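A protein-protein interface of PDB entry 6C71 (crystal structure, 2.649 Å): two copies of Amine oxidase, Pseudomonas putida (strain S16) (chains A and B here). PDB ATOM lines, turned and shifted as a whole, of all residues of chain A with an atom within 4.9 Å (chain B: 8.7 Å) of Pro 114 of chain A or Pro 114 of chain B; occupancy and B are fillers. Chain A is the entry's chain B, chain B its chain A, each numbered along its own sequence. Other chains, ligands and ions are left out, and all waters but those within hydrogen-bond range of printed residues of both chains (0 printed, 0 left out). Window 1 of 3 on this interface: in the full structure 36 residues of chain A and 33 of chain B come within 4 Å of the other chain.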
ATOM      1  N   TRP A 111     -11.360  24.726  19.924  1.00  0.00           N
ATOM      2  CA  TRP A 111     -10.870  23.500  20.545  1.00  0.00           C
ATOM      3  C   TRP A 111     -10.256  23.733  21.918  1.00  0.00           C
ATOM      4  O   TRP A 111     -10.032  22.762  22.648  1.00  0.00           O
ATOM      5  CB  TRP A 111      -9.854  22.801  19.635  1.00  0.00           C
ATOM      6  CG  TRP A 111      -8.803  23.691  19.058  1.00  0.00           C
ATOM      7  CD1 TRP A 111      -7.583  23.974  19.600  1.00  0.00           C
ATOM      8  CD2 TRP A 111      -8.867  24.405  17.817  1.00  0.00           C
ATOM      9  NE1 TRP A 111      -6.886  24.824  18.778  1.00  0.00           N
ATOM     10  CE2 TRP A 111      -7.651  25.105  17.676  1.00  0.00           C
ATOM     11  CE3 TRP A 111      -9.833  24.525  16.814  1.00  0.00           C
ATOM     12  CZ2 TRP A 111      -7.378  25.912  16.575  1.00  0.00           C
ATOM     13  CZ3 TRP A 111      -9.560  25.327  15.721  1.00  0.00           C
ATOM     14  CH2 TRP A 111      -8.342  26.009  15.610  1.00  0.00           C
ATOM     15  N   LEU A 112      -9.977  24.982  22.286  1.00  0.00           N
ATOM     16  CA  LEU A 112      -9.577  25.295  23.652  1.00  0.00           C
ATOM     17  C   LEU A 112     -10.767  25.372  24.596  1.00  0.00           C
ATOM     18  O   LEU A 112     -10.577  25.598  25.797  1.00  0.00           O
ATOM     19  CB  LEU A 112      -8.796  26.611  23.688  1.00  0.00           C
ATOM     20  CG  LEU A 112      -7.435  26.596  22.990  1.00  0.00           C
ATOM     21  CD1 LEU A 112      -6.843  27.993  22.942  1.00  0.00           C
ATOM     22  CD2 LEU A 112      -6.489  25.633  23.691  1.00  0.00           C
ATOM     23  N   GLN A 113     -11.984  25.193  24.080  1.00  0.00           N
ATOM     24  CA  GLN A 113     -13.193  25.106  24.883  1.00  0.00           C
ATOM     25  C   GLN A 113     -13.548  23.633  25.029  1.00  0.00           C
ATOM     26  O   GLN A 113     -14.058  23.024  24.077  1.00  0.00           O
ATOM     27  CB  GLN A 113     -14.334  25.889  24.227  1.00  0.00           C
ATOM     28  CG  GLN A 113     -13.948  27.333  23.922  1.00  0.00           C
ATOM     29  CD  GLN A 113     -15.037  28.116  23.215  1.00  0.00           C
ATOM     30  OE1 GLN A 113     -15.769  27.578  22.387  1.00  0.00           O
ATOM     31  NE2 GLN A 113     -15.141  29.401  23.536  1.00  0.00           N
ATOM     32  N   PRO A 114     -13.301  23.018  26.190  1.00  0.00           N
ATOM     33  CA  PRO A 114     -13.243  21.545  26.240  1.00  0.00           C
ATOM     34  C   PRO A 114     -14.569  20.849  25.986  1.00  0.00           C
ATOM     35  O   PRO A 114     -14.608  19.855  25.250  1.00  0.00           O
ATOM     36  CB  PRO A 114     -12.725  21.267  27.660  1.00  0.00           C
ATOM     37  CG  PRO A 114     -13.051  22.494  28.445  1.00  0.00           C
ATOM     38  CD  PRO A 114     -12.994  23.643  27.488  1.00  0.00           C
ATOM     39  N   HIS A 115     -15.657  21.334  26.581  1.00  0.00           N
ATOM     40  CA  HIS A 115     -16.910  20.585  26.563  1.00  0.00           C
ATOM     41  C   HIS A 115     -17.518  20.546  25.164  1.00  0.00           C
ATOM     42  O   HIS A 115     -17.803  19.465  24.627  1.00  0.00           O
ATOM     43  CB  HIS A 115     -17.871  21.201  27.579  1.00  0.00           C
ATOM     44  CG  HIS A 115     -17.214  21.547  28.880  1.00  0.00           C
ATOM     45  ND1 HIS A 115     -16.633  22.775  29.116  1.00  0.00           N
ATOM     46  CD2 HIS A 115     -17.028  20.821  30.008  1.00  0.00           C
ATOM     47  CE1 HIS A 115     -16.123  22.793  30.335  1.00  0.00           C
ATOM     48  NE2 HIS A 115     -16.351  21.620  30.899  1.00  0.00           N
ATOM     49  N   VAL A 116     -17.707  21.716  24.547  1.00  0.00           N
ATOM     50  CA  VAL A 116     -18.298  21.762  23.213  1.00  0.00           C
ATOM     51  C   VAL A 116     -17.401  21.070  22.194  1.00  0.00           C
ATOM     52  O   VAL A 116     -17.895  20.450  21.244  1.00  0.00           O
ATOM     53  CB  VAL A 116     -18.608  23.221  22.811  1.00  0.00           C
ATOM     54  CG1 VAL A 116     -17.329  24.032  22.651  1.00  0.00           C
ATOM     55  CG2 VAL A 116     -19.433  23.254  21.532  1.00  0.00           C
ATOM     56  N   TRP A 117     -16.079  21.148  22.373  1.00  0.00           N
ATOM     57  CA  TRP A 117     -15.185  20.481  21.432  1.00  0.00           C
ATOM     58  C   TRP A 117     -15.269  18.969  21.576  1.00  0.00           C
ATOM     59  O   TRP A 117     -15.201  18.241  20.579  1.00  0.00           O
ATOM     60  CB  TRP A 117     -13.747  20.957  21.621  1.00  0.00           C
ATOM     61  CG  TRP A 117     -12.876  20.548  20.481  1.00  0.00           C
ATOM     62  CD1 TRP A 117     -11.975  19.525  20.459  1.00  0.00           C
ATOM     63  CD2 TRP A 117     -12.851  21.135  19.176  1.00  0.00           C
ATOM     64  NE1 TRP A 117     -11.375  19.451  19.223  1.00  0.00           N
ATOM     65  CE2 TRP A 117     -11.898  20.428  18.417  1.00  0.00           C
ATOM     66  CE3 TRP A 117     -13.533  22.199  18.579  1.00  0.00           C
ATOM     67  CZ2 TRP A 117     -11.610  20.750  17.094  1.00  0.00           C
ATOM     68  CZ3 TRP A 117     -13.248  22.517  17.267  1.00  0.00           C
ATOM     69  CH2 TRP A 117     -12.295  21.795  16.538  1.00  0.00           C
ATOM     70  N   ALA A 118     -15.390  18.477  22.811  1.00  0.00           N
ATOM     71  CA  ALA A 118     -15.617  17.050  23.011  1.00  0.00           C
ATOM     72  C   ALA A 118     -16.919  16.611  22.356  1.00  0.00           C
ATOM     73  O   ALA A 118     -16.990  15.529  21.761  1.00  0.00           O
ATOM     74  CB  ALA A 118     -15.624  16.717  24.500  1.00  0.00           C
ATOM     75  N   HIS A 178     -11.267  27.201  35.972  1.00  0.00           N
ATOM     76  CA  HIS A 178     -12.488  26.440  36.204  1.00  0.00           C
ATOM     77  C   HIS A 178     -12.832  26.284  37.673  1.00  0.00           C
ATOM     78  O   HIS A 178     -13.828  25.627  37.996  1.00  0.00           O
ATOM     79  CB  HIS A 178     -12.382  25.062  35.534  1.00  0.00           C
ATOM     80  CG  HIS A 178     -12.471  25.119  34.040  1.00  0.00           C
ATOM     81  ND1 HIS A 178     -11.388  25.402  33.234  1.00  0.00           N
ATOM     82  CD2 HIS A 178     -13.525  24.947  33.210  1.00  0.00           C
ATOM     83  CE1 HIS A 178     -11.772  25.383  31.969  1.00  0.00           C
ATOM     84  NE2 HIS A 178     -13.064  25.112  31.929  1.00  0.00           N
ATOM     85  N   TRP A 459     -16.240  28.830  30.484  1.00  0.00           N
ATOM     86  CA  TRP A 459     -16.636  29.747  29.416  1.00  0.00           C
ATOM     87  C   TRP A 459     -18.095  30.159  29.624  1.00  0.00           C
ATOM     88  O   TRP A 459     -19.003  29.790  28.876  1.00  0.00           O
ATOM     89  CB  TRP A 459     -16.421  29.100  28.055  1.00  0.00           C
ATOM     90  CG  TRP A 459     -14.991  28.736  27.792  1.00  0.00           C
ATOM     91  CD1 TRP A 459     -14.362  27.578  28.145  1.00  0.00           C
ATOM     92  CD2 TRP A 459     -14.008  29.542  27.133  1.00  0.00           C
ATOM     93  NE1 TRP A 459     -13.050  27.609  27.738  1.00  0.00           N
ATOM     94  CE2 TRP A 459     -12.807  28.805  27.116  1.00  0.00           C
ATOM     95  CE3 TRP A 459     -14.027  30.814  26.553  1.00  0.00           C
ATOM     96  CZ2 TRP A 459     -11.637  29.297  26.541  1.00  0.00           C
ATOM     97  CZ3 TRP A 459     -12.865  31.301  25.983  1.00  0.00           C
ATOM     98  CH2 TRP A 459     -11.686  30.544  25.981  1.00  0.00           C
ATOM     99  N   ASP A 464     -19.794  26.732  25.263  1.00  0.00           N
ATOM    100  CA  ASP A 464     -19.082  25.725  26.041  1.00  0.00           C
ATOM    101  C   ASP A 464     -19.523  25.732  27.499  1.00  0.00           C
ATOM    102  O   ASP A 464     -19.632  24.671  28.124  1.00  0.00           O
ATOM    103  CB  ASP A 464     -17.574  25.954  25.935  1.00  0.00           C
ATOM    104  CG  ASP A 464     -16.778  24.980  26.780  1.00  0.00           C
ATOM    105  OD1 ASP A 464     -16.571  25.263  27.980  1.00  0.00           O
ATOM    106  OD2 ASP A 464     -16.362  23.930  26.246  1.00  0.00           O
ATOM    107  N   HIS B 110      -4.992  18.515  31.946  1.00  0.00           N
ATOM    108  CA  HIS B 110      -5.172  19.961  31.954  1.00  0.00           C
ATOM    109  C   HIS B 110      -6.499  20.291  31.287  1.00  0.00           C
ATOM    110  O   HIS B 110      -7.026  19.508  30.492  1.00  0.00           O
ATOM    111  CB  HIS B 110      -4.012  20.665  31.242  1.00  0.00           C
ATOM    112  CG  HIS B 110      -3.875  22.115  31.587  1.00  0.00           C
ATOM    113  ND1 HIS B 110      -4.424  23.120  30.819  1.00  0.00           N
ATOM    114  CD2 HIS B 110      -3.244  22.730  32.615  1.00  0.00           C
ATOM    115  CE1 HIS B 110      -4.139  24.290  31.360  1.00  0.00           C
ATOM    116  NE2 HIS B 110      -3.424  24.082  32.451  1.00  0.00           N
ATOM    117  N   TRP B 111      -7.033  21.468  31.622  1.00  0.00           N
ATOM    118  CA  TRP B 111      -8.305  21.903  31.056  1.00  0.00           C
ATOM    119  C   TRP B 111      -8.185  22.389  29.618  1.00  0.00           C
ATOM    120  O   TRP B 111      -9.213  22.544  28.949  1.00  0.00           O
ATOM    121  CB  TRP B 111      -8.929  23.004  31.921  1.00  0.00           C
ATOM    122  CG  TRP B 111      -7.977  24.080  32.332  1.00  0.00           C
ATOM    123  CD1 TRP B 111      -7.707  25.237  31.664  1.00  0.00           C
ATOM    124  CD2 TRP B 111      -7.174  24.106  33.519  1.00  0.00           C
ATOM    125  NE1 TRP B 111      -6.782  25.981  32.357  1.00  0.00           N
ATOM    126  CE2 TRP B 111      -6.439  25.307  33.499  1.00  0.00           C
ATOM    127  CE3 TRP B 111      -7.005  23.227  34.593  1.00  0.00           C
ATOM    128  CZ2 TRP B 111      -5.546  25.652  34.512  1.00  0.00           C
ATOM    129  CZ3 TRP B 111      -6.119  23.572  35.598  1.00  0.00           C
ATOM    130  CH2 TRP B 111      -5.403  24.774  35.551  1.00  0.00           C
ATOM    131  N   LEU B 112      -6.971  22.630  29.126  1.00  0.00           N
ATOM    132  CA  LEU B 112      -6.771  22.924  27.713  1.00  0.00           C
ATOM    133  C   LEU B 112      -6.763  21.668  26.853  1.00  0.00           C
ATOM    134  O   LEU B 112      -6.643  21.772  25.628  1.00  0.00           O
ATOM    135  CB  LEU B 112      -5.465  23.697  27.519  1.00  0.00           C
ATOM    136  CG  LEU B 112      -5.440  25.095  28.140  1.00  0.00           C
ATOM    137  CD1 LEU B 112      -4.049  25.703  28.042  1.00  0.00           C
ATOM    138  CD2 LEU B 112      -6.476  25.997  27.486  1.00  0.00           C
ATOM    139  N   GLN B 113      -6.891  20.493  27.468  1.00  0.00           N
ATOM    140  CA  GLN B 113      -7.029  19.228  26.764  1.00  0.00           C
ATOM    141  C   GLN B 113      -8.508  18.869  26.758  1.00  0.00           C
ATOM    142  O   GLN B 113      -9.038  18.427  27.790  1.00  0.00           O
ATOM    143  CB  GLN B 113      -6.199  18.140  27.447  1.00  0.00           C
ATOM    144  CG  GLN B 113      -4.739  18.550  27.629  1.00  0.00           C
ATOM    145  CD  GLN B 113      -3.909  17.517  28.365  1.00  0.00           C
ATOM    146  OE1 GLN B 113      -4.393  16.849  29.278  1.00  0.00           O
ATOM    147  NE2 GLN B 113      -2.644  17.394  27.979  1.00  0.00           N
ATOM    148  N   PRO B 114      -9.215  19.036  25.636  1.00  0.00           N
ATOM    149  CA  PRO B 114     -10.686  19.105  25.706  1.00  0.00           C
ATOM    150  C   PRO B 114     -11.364  17.814  26.128  1.00  0.00           C
ATOM    151  O   PRO B 114     -12.286  17.849  26.954  1.00  0.00           O
ATOM    152  CB  PRO B 114     -11.082  19.508  24.276  1.00  0.00           C
ATOM    153  CG  PRO B 114      -9.927  19.108  23.421  1.00  0.00           C
ATOM    154  CD  PRO B 114      -8.701  19.231  24.269  1.00  0.00           C
ATOM    155  N   HIS B 115     -10.944  16.675  25.583  1.00  0.00           N
ATOM    156  CA  HIS B 115     -11.695  15.439  25.784  1.00  0.00           C
ATOM    157  C   HIS B 115     -11.589  14.949  27.225  1.00  0.00           C
ATOM    158  O   HIS B 115     -12.610  14.697  27.883  1.00  0.00           O
ATOM    159  CB  HIS B 115     -11.210  14.388  24.787  1.00  0.00           C
ATOM    160  CG  HIS B 115     -11.025  14.927  23.401  1.00  0.00           C
ATOM    161  ND1 HIS B 115      -9.830  15.456  22.960  1.00  0.00           N
ATOM    162  CD2 HIS B 115     -11.894  15.052  22.369  1.00  0.00           C
ATOM    163  CE1 HIS B 115      -9.966  15.866  21.711  1.00  0.00           C
ATOM    164  NE2 HIS B 115     -11.209  15.633  21.330  1.00  0.00           N
ATOM    165  N   VAL B 116     -10.364  14.815  27.741  1.00  0.00           N
ATOM    166  CA  VAL B 116     -10.192  14.332  29.109  1.00  0.00           C
ATOM    167  C   VAL B 116     -10.807  15.303  30.112  1.00  0.00           C
ATOM    168  O   VAL B 116     -11.347  14.881  31.145  1.00  0.00           O
ATOM    169  CB  VAL B 116      -8.700  14.065  29.404  1.00  0.00           C
ATOM    170  CG1 VAL B 116      -7.895  15.359  29.399  1.00  0.00           C
ATOM    171  CG2 VAL B 116      -8.542  13.333  30.729  1.00  0.00           C
ATOM    172  N   TRP B 117     -10.761  16.607  29.826  1.00  0.00           N
ATOM    173  CA  TRP B 117     -11.370  17.567  30.740  1.00  0.00           C
ATOM    174  C   TRP B 117     -12.887  17.462  30.717  1.00  0.00           C
ATOM    175  O   TRP B 117     -13.540  17.600  31.758  1.00  0.00           O
ATOM    176  CB  TRP B 117     -10.933  18.993  30.410  1.00  0.00           C
ATOM    177  CG  TRP B 117     -11.304  19.952  31.500  1.00  0.00           C
ATOM    178  CD1 TRP B 117     -12.342  20.839  31.494  1.00  0.00           C
ATOM    179  CD2 TRP B 117     -10.667  20.088  32.775  1.00  0.00           C
ATOM    180  NE1 TRP B 117     -12.375  21.535  32.679  1.00  0.00           N
ATOM    181  CE2 TRP B 117     -11.358  21.091  33.484  1.00  0.00           C
ATOM    182  CE3 TRP B 117      -9.571  19.467  33.381  1.00  0.00           C
ATOM    183  CZ2 TRP B 117     -10.989  21.487  34.768  1.00  0.00           C
ATOM    184  CZ3 TRP B 117      -9.206  19.861  34.657  1.00  0.00           C
ATOM    185  CH2 TRP B 117      -9.914  20.860  35.336  1.00  0.00           C
ATOM    186  N   ALA B 118     -13.468  17.240  29.536  1.00  0.00           N
ATOM    187  CA  ALA B 118     -14.907  17.009  29.465  1.00  0.00           C
ATOM    188  C   ALA B 118     -15.304  15.767  30.252  1.00  0.00           C
ATOM    189  O   ALA B 118     -16.328  15.765  30.944  1.00  0.00           O
ATOM    190  CB  ALA B 118     -15.349  16.889  28.009  1.00  0.00           C
ATOM    191  N   GLU B 119     -14.503  14.700  30.161  1.00  0.00           N
ATOM    192  CA  GLU B 119     -14.794  13.506  30.952  1.00  0.00           C
ATOM    193  C   GLU B 119     -14.705  13.797  32.446  1.00  0.00           C
ATOM    194  O   GLU B 119     -15.541  13.327  33.232  1.00  0.00           O
ATOM    195  CB  GLU B 119     -13.849  12.370  30.562  1.00  0.00           C
ATOM    196  CG  GLU B 119     -13.951  11.950  29.101  1.00  0.00           C
ATOM    197  CD  GLU B 119     -15.343  11.472  28.719  1.00  0.00           C
ATOM    198  OE1 GLU B 119     -16.076  10.975  29.601  1.00  0.00           O
ATOM    199  OE2 GLU B 119     -15.706  11.593  27.530  1.00  0.00           O
ATOM    200  N   MET B 120     -13.703  14.580  32.858  1.00  0.00           N
ATOM    201  CA  MET B 120     -13.582  14.928  34.271  1.00  0.00           C
ATOM    202  C   MET B 120     -14.773  15.756  34.731  1.00  0.00           C
ATOM    203  O   MET B 120     -15.236  15.616  35.870  1.00  0.00           O
ATOM    204  CB  MET B 120     -12.279  15.685  34.527  1.00  0.00           C
ATOM    205  CG  MET B 120     -11.074  14.796  34.771  1.00  0.00           C
ATOM    206  SD  MET B 120      -9.523  15.670  34.506  1.00  0.00           S
ATOM    207  CE  MET B 120      -9.238  16.348  36.140  1.00  0.00           C
ATOM    208  N   GLN B 121     -15.283  16.628  33.858  1.00  0.00           N
ATOM    209  CA  GLN B 121     -16.488  17.379  34.184  1.00  0.00           C
ATOM    210  C   GLN B 121     -17.688  16.453  34.326  1.00  0.00           C
ATOM    211  O   GLN B 121     -18.499  16.609  35.246  1.00  0.00           O
ATOM    212  CB  GLN B 121     -16.751  18.434  33.110  1.00  0.00           C
ATOM    213  CG  GLN B 121     -18.038  19.211  33.309  1.00  0.00           C
ATOM    214  CD  GLN B 121     -18.006  20.053  34.567  1.00  0.00           C
ATOM    215  OE1 GLN B 121     -18.941  20.030  35.369  1.00  0.00           O
ATOM    216  NE2 GLN B 121     -16.929  20.806  34.746  1.00  0.00           N
ATOM    217  N   ARG B 122     -17.815  15.479  33.422  1.00  0.00           N
ATOM    218  CA  ARG B 122     -18.955  14.569  33.458  1.00  0.00           C
ATOM    219  C   ARG B 122     -18.964  13.742  34.737  1.00  0.00           C
ATOM    220  O   ARG B 122     -20.006  13.590  35.385  1.00  0.00           O
ATOM    221  CB  ARG B 122     -18.935  13.652  32.235  1.00  0.00           C
ATOM    222  CG  ARG B 122     -19.739  12.372  32.418  1.00  0.00           C
ATOM    223  CD  ARG B 122     -20.227  11.829  31.088  1.00  0.00           C
ATOM    224  NE  ARG B 122     -19.274  12.092  30.016  1.00  0.00           N
ATOM    225  CZ  ARG B 122     -19.568  12.741  28.894  1.00  0.00           C
ATOM    226  NH1 ARG B 122     -20.797  13.195  28.691  1.00  0.00           N
ATOM    227  NH2 ARG B 122     -18.634  12.934  27.974  1.00  0.00           N
ATOM    228  N   HIS B 178      -5.800  20.265  15.422  1.00  0.00           N
ATOM    229  CA  HIS B 178      -6.561  19.025  15.332  1.00  0.00           C
ATOM    230  C   HIS B 178      -6.766  18.554  13.896  1.00  0.00           C
ATOM    231  O   HIS B 178      -7.414  17.523  13.685  1.00  0.00           O
ATOM    232  CB  HIS B 178      -7.913  19.188  16.037  1.00  0.00           C
ATOM    233  CG  HIS B 178      -7.812  19.224  17.532  1.00  0.00           C
ATOM    234  ND1 HIS B 178      -7.484  20.367  18.229  1.00  0.00           N
ATOM    235  CD2 HIS B 178      -7.981  18.253  18.461  1.00  0.00           C
ATOM    236  CE1 HIS B 178      -7.460  20.100  19.522  1.00  0.00           C
ATOM    237  NE2 HIS B 178      -7.759  18.824  19.690  1.00  0.00           N
ATOM    238  N   CYS B 237      -1.475  22.795  20.260  1.00  0.00           N
ATOM    239  CA  CYS B 237      -2.623  22.356  21.045  1.00  0.00           C
ATOM    240  C   CYS B 237      -2.718  23.105  22.368  1.00  0.00           C
ATOM    241  O   CYS B 237      -3.817  23.280  22.906  1.00  0.00           O
ATOM    242  CB  CYS B 237      -2.541  20.849  21.293  1.00  0.00           C
ATOM    243  SG  CYS B 237      -3.020  19.820  19.886  1.00  0.00           S
ATOM    244  N   GLY B 238      -1.586  23.555  22.904  1.00  0.00           N
ATOM    245  CA  GLY B 238      -1.575  24.259  24.170  1.00  0.00           C
ATOM    246  C   GLY B 238      -1.663  25.765  24.026  1.00  0.00           C
ATOM    247  O   GLY B 238      -1.170  26.505  24.881  1.00  0.00           O
ATOM    248  N   GLY B 458      -4.966  15.217  18.001  1.00  0.00           N
ATOM    249  CA  GLY B 458      -4.545  16.277  18.898  1.00  0.00           C
ATOM    250  C   GLY B 458      -3.420  15.893  19.837  1.00  0.00           C
ATOM    251  O   GLY B 458      -2.265  15.771  19.420  1.00  0.00           O
ATOM    252  N   TRP B 459      -3.748  15.698  21.115  1.00  0.00           N
ATOM    253  CA  TRP B 459      -2.754  15.396  22.146  1.00  0.00           C
ATOM    254  C   TRP B 459      -2.348  13.923  22.054  1.00  0.00           C
ATOM    255  O   TRP B 459      -2.663  13.095  22.910  1.00  0.00           O
ATOM    256  CB  TRP B 459      -3.305  15.737  23.523  1.00  0.00           C
ATOM    257  CG  TRP B 459      -3.629  17.188  23.707  1.00  0.00           C
ATOM    258  CD1 TRP B 459      -4.789  17.820  23.367  1.00  0.00           C
ATOM    259  CD2 TRP B 459      -2.787  18.184  24.298  1.00  0.00           C
ATOM    260  NE1 TRP B 459      -4.717  19.153  23.700  1.00  0.00           N
ATOM    261  CE2 TRP B 459      -3.498  19.400  24.275  1.00  0.00           C
ATOM    262  CE3 TRP B 459      -1.498  18.167  24.842  1.00  0.00           C
ATOM    263  CZ2 TRP B 459      -2.964  20.588  24.774  1.00  0.00           C
ATOM    264  CZ3 TRP B 459      -0.970  19.347  25.336  1.00  0.00           C
ATOM    265  CH2 TRP B 459      -1.702  20.540  25.299  1.00  0.00           C
ATOM    266  N   ASP B 464      -5.455  12.599  26.771  1.00  0.00           N
ATOM    267  CA  ASP B 464      -6.513  13.247  26.006  1.00  0.00           C
ATOM    268  C   ASP B 464      -6.609  12.680  24.595  1.00  0.00           C
ATOM    269  O   ASP B 464      -7.710  12.529  24.054  1.00  0.00           O
ATOM    270  CB  ASP B 464      -6.272  14.756  25.959  1.00  0.00           C
ATOM    271  CG  ASP B 464      -7.298  15.484  25.118  1.00  0.00           C
ATOM    272  OD1 ASP B 464      -8.355  15.861  25.666  1.00  0.00           O
ATOM    273  OD2 ASP B 464      -7.048  15.678  23.909  1.00  0.00           O
ATOM    274  N   GLY B 465      -5.467  12.374  23.977  1.00  0.00           N
ATOM    275  CA  GLY B 465      -5.498  11.765  22.656  1.00  0.00           C
ATOM    276  C   GLY B 465      -6.166  10.404  22.658  1.00  0.00           C
ATOM    277  O   GLY B 465      -6.941  10.079  21.754  1.00  0.00           O
ATOM    278  N   VAL B 467      -8.476   9.393  24.801  1.00  0.00           N
ATOM    279  CA  VAL B 467      -9.908   9.624  24.980  1.00  0.00           C
ATOM    280  C   VAL B 467     -10.548  10.074  23.670  1.00  0.00           C
ATOM    281  O   VAL B 467     -11.633   9.605  23.295  1.00  0.00           O
ATOM    282  CB  VAL B 467     -10.145  10.642  26.111  1.00  0.00           C
ATOM    283  CG1 VAL B 467     -11.625  10.960  26.242  1.00  0.00           C
ATOM    284  CG2 VAL B 467      -9.591  10.110  27.425  1.00  0.00           C
ATOM    285  N   GLU B 468      -9.884  10.981  22.950  1.00  0.00           N
ATOM    286  CA  GLU B 468     -10.396  11.450  21.664  1.00  0.00           C
ATOM    287  C   GLU B 468     -10.565  10.293  20.686  1.00  0.00           C
ATOM    288  O   GLU B 468     -11.623  10.141  20.056  1.00  0.00           O
ATOM    289  CB  GLU B 468      -9.458  12.511  21.087  1.00  0.00           C
ATOM    290  CG  GLU B 468      -9.675  12.802  19.611  1.00  0.00           C
ATOM    291  CD  GLU B 468      -8.412  13.285  18.918  1.00  0.00           C
ATOM    292  OE1 GLU B 468      -7.639  14.041  19.546  1.00  0.00           O
ATOM    293  OE2 GLU B 468      -8.193  12.910  17.747  1.00  0.00           O
ATOM    294  N   LEU B 471     -13.620   8.404  21.493  1.00  0.00           N
ATOM    295  CA  LEU B 471     -14.851   9.039  21.031  1.00  0.00           C
ATOM    296  C   LEU B 471     -15.067   8.795  19.541  1.00  0.00           C
ATOM    297  O   LEU B 471     -16.168   8.426  19.109  1.00  0.00           O
ATOM    298  CB  LEU B 471     -14.807  10.539  21.331  1.00  0.00           C
ATOM    299  CG  LEU B 471     -14.707  10.960  22.800  1.00  0.00           C
ATOM    300  CD1 LEU B 471     -14.522  12.466  22.914  1.00  0.00           C
ATOM    301  CD2 LEU B 471     -15.937  10.514  23.575  1.00  0.00           C
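ND1 of His 110 of chain B is in hydrogen-bond range of N of Leu 112 of chain B, at 3.1 Å.
The backbone NH of His 115 of chain A is in hydrogen-bond range of the side-chain carboxylate of Asp 464 of chain A (2.7 Å).
Among the printed residues, merely in contact across the chains: Pro 114 of chain A with Pro 114 of chain B (3.5 Å), Ala 118 of chain A with Ala 118 of chain B (3.5 Å), Pro 114 of chain A with Trp 117 of chain B (3.5 Å), Trp 111 of chain A with His 178 of chain B (3.6 Å), Trp 117 of chain A with Pro 114 of chain B (3.6 Å), His 178 of chain A with Trp 117 of chain B (3.6 Å), Leu 112 of chain A with Cys 237 of chain B (3.6 Å), His 178 of chain A with Trp 111 of chain B (3.7 Å), Trp 117 of chain A with His 178 of chain B (3.7 Å), Trp 111 of chain A with Pro 114 of chain B (3.7 Å), His 115 of chain A with Gln 121 of chain B (3.8 Å), Leu 112 of chain A with Leu 112 of chain B (3.8 Å) and Pro 114 of chain A with Trp 111 of chain B (3.9 Å).
Of the printed residues of chain B, Trp 111 of chain A touches Pro 114 and His 178.
Of chain A, only Trp 111 (3.7 Å), Pro 114 (3.5 Å) and Trp 117 (3.6 Å) come within 4 Å of Pro 114 of chain B.
Printed residues of chain A within 4 Å of Gln 121 of chain B: His 115 (3.8 Å).
Printed residues of chain A within 4 Å of His 178 of chain B: Trp 111 (3.6 Å) and Trp 117 (3.7 Å).
Val 467 of chain B touches none of the printed residues of chain A.
The nearest residue of chain B that does not touch Pro 114 of chain A is Ala 118 of chain B (4.1 Å).
Of the 23 printed residues of chain B, 8 touch a printed residue of chain A.
Hydrophobic or aromatic side chains of chain B that line the printed part of chain A: Trp 111, Leu 112, Pro 114, Trp 117, Ala 118 and His 178.
Among the printed residues, 13 pairs touch across the chains.
Trp 111 of chain A touches Pro 114 of chain B, and with the chains exchanged Pro 114 of chain A touches Trp 111 of chain B.
Trp 111 of chain A touches His 178 of chain B, and with the chains exchanged His 178 of chain A touches Trp 111 of chain B.
Leu 112 of chain B touches its own counterpart, Leu 112 of chain A.
Pro 114 of chain A touches Trp 117 of chain B, and with the chains exchanged Trp 117 of chain A touches Pro 114 of chain B.
Positions printed for both chains: 111, 112, 113, 114, 115, 116, 117, 118, 178, 459 and 464.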
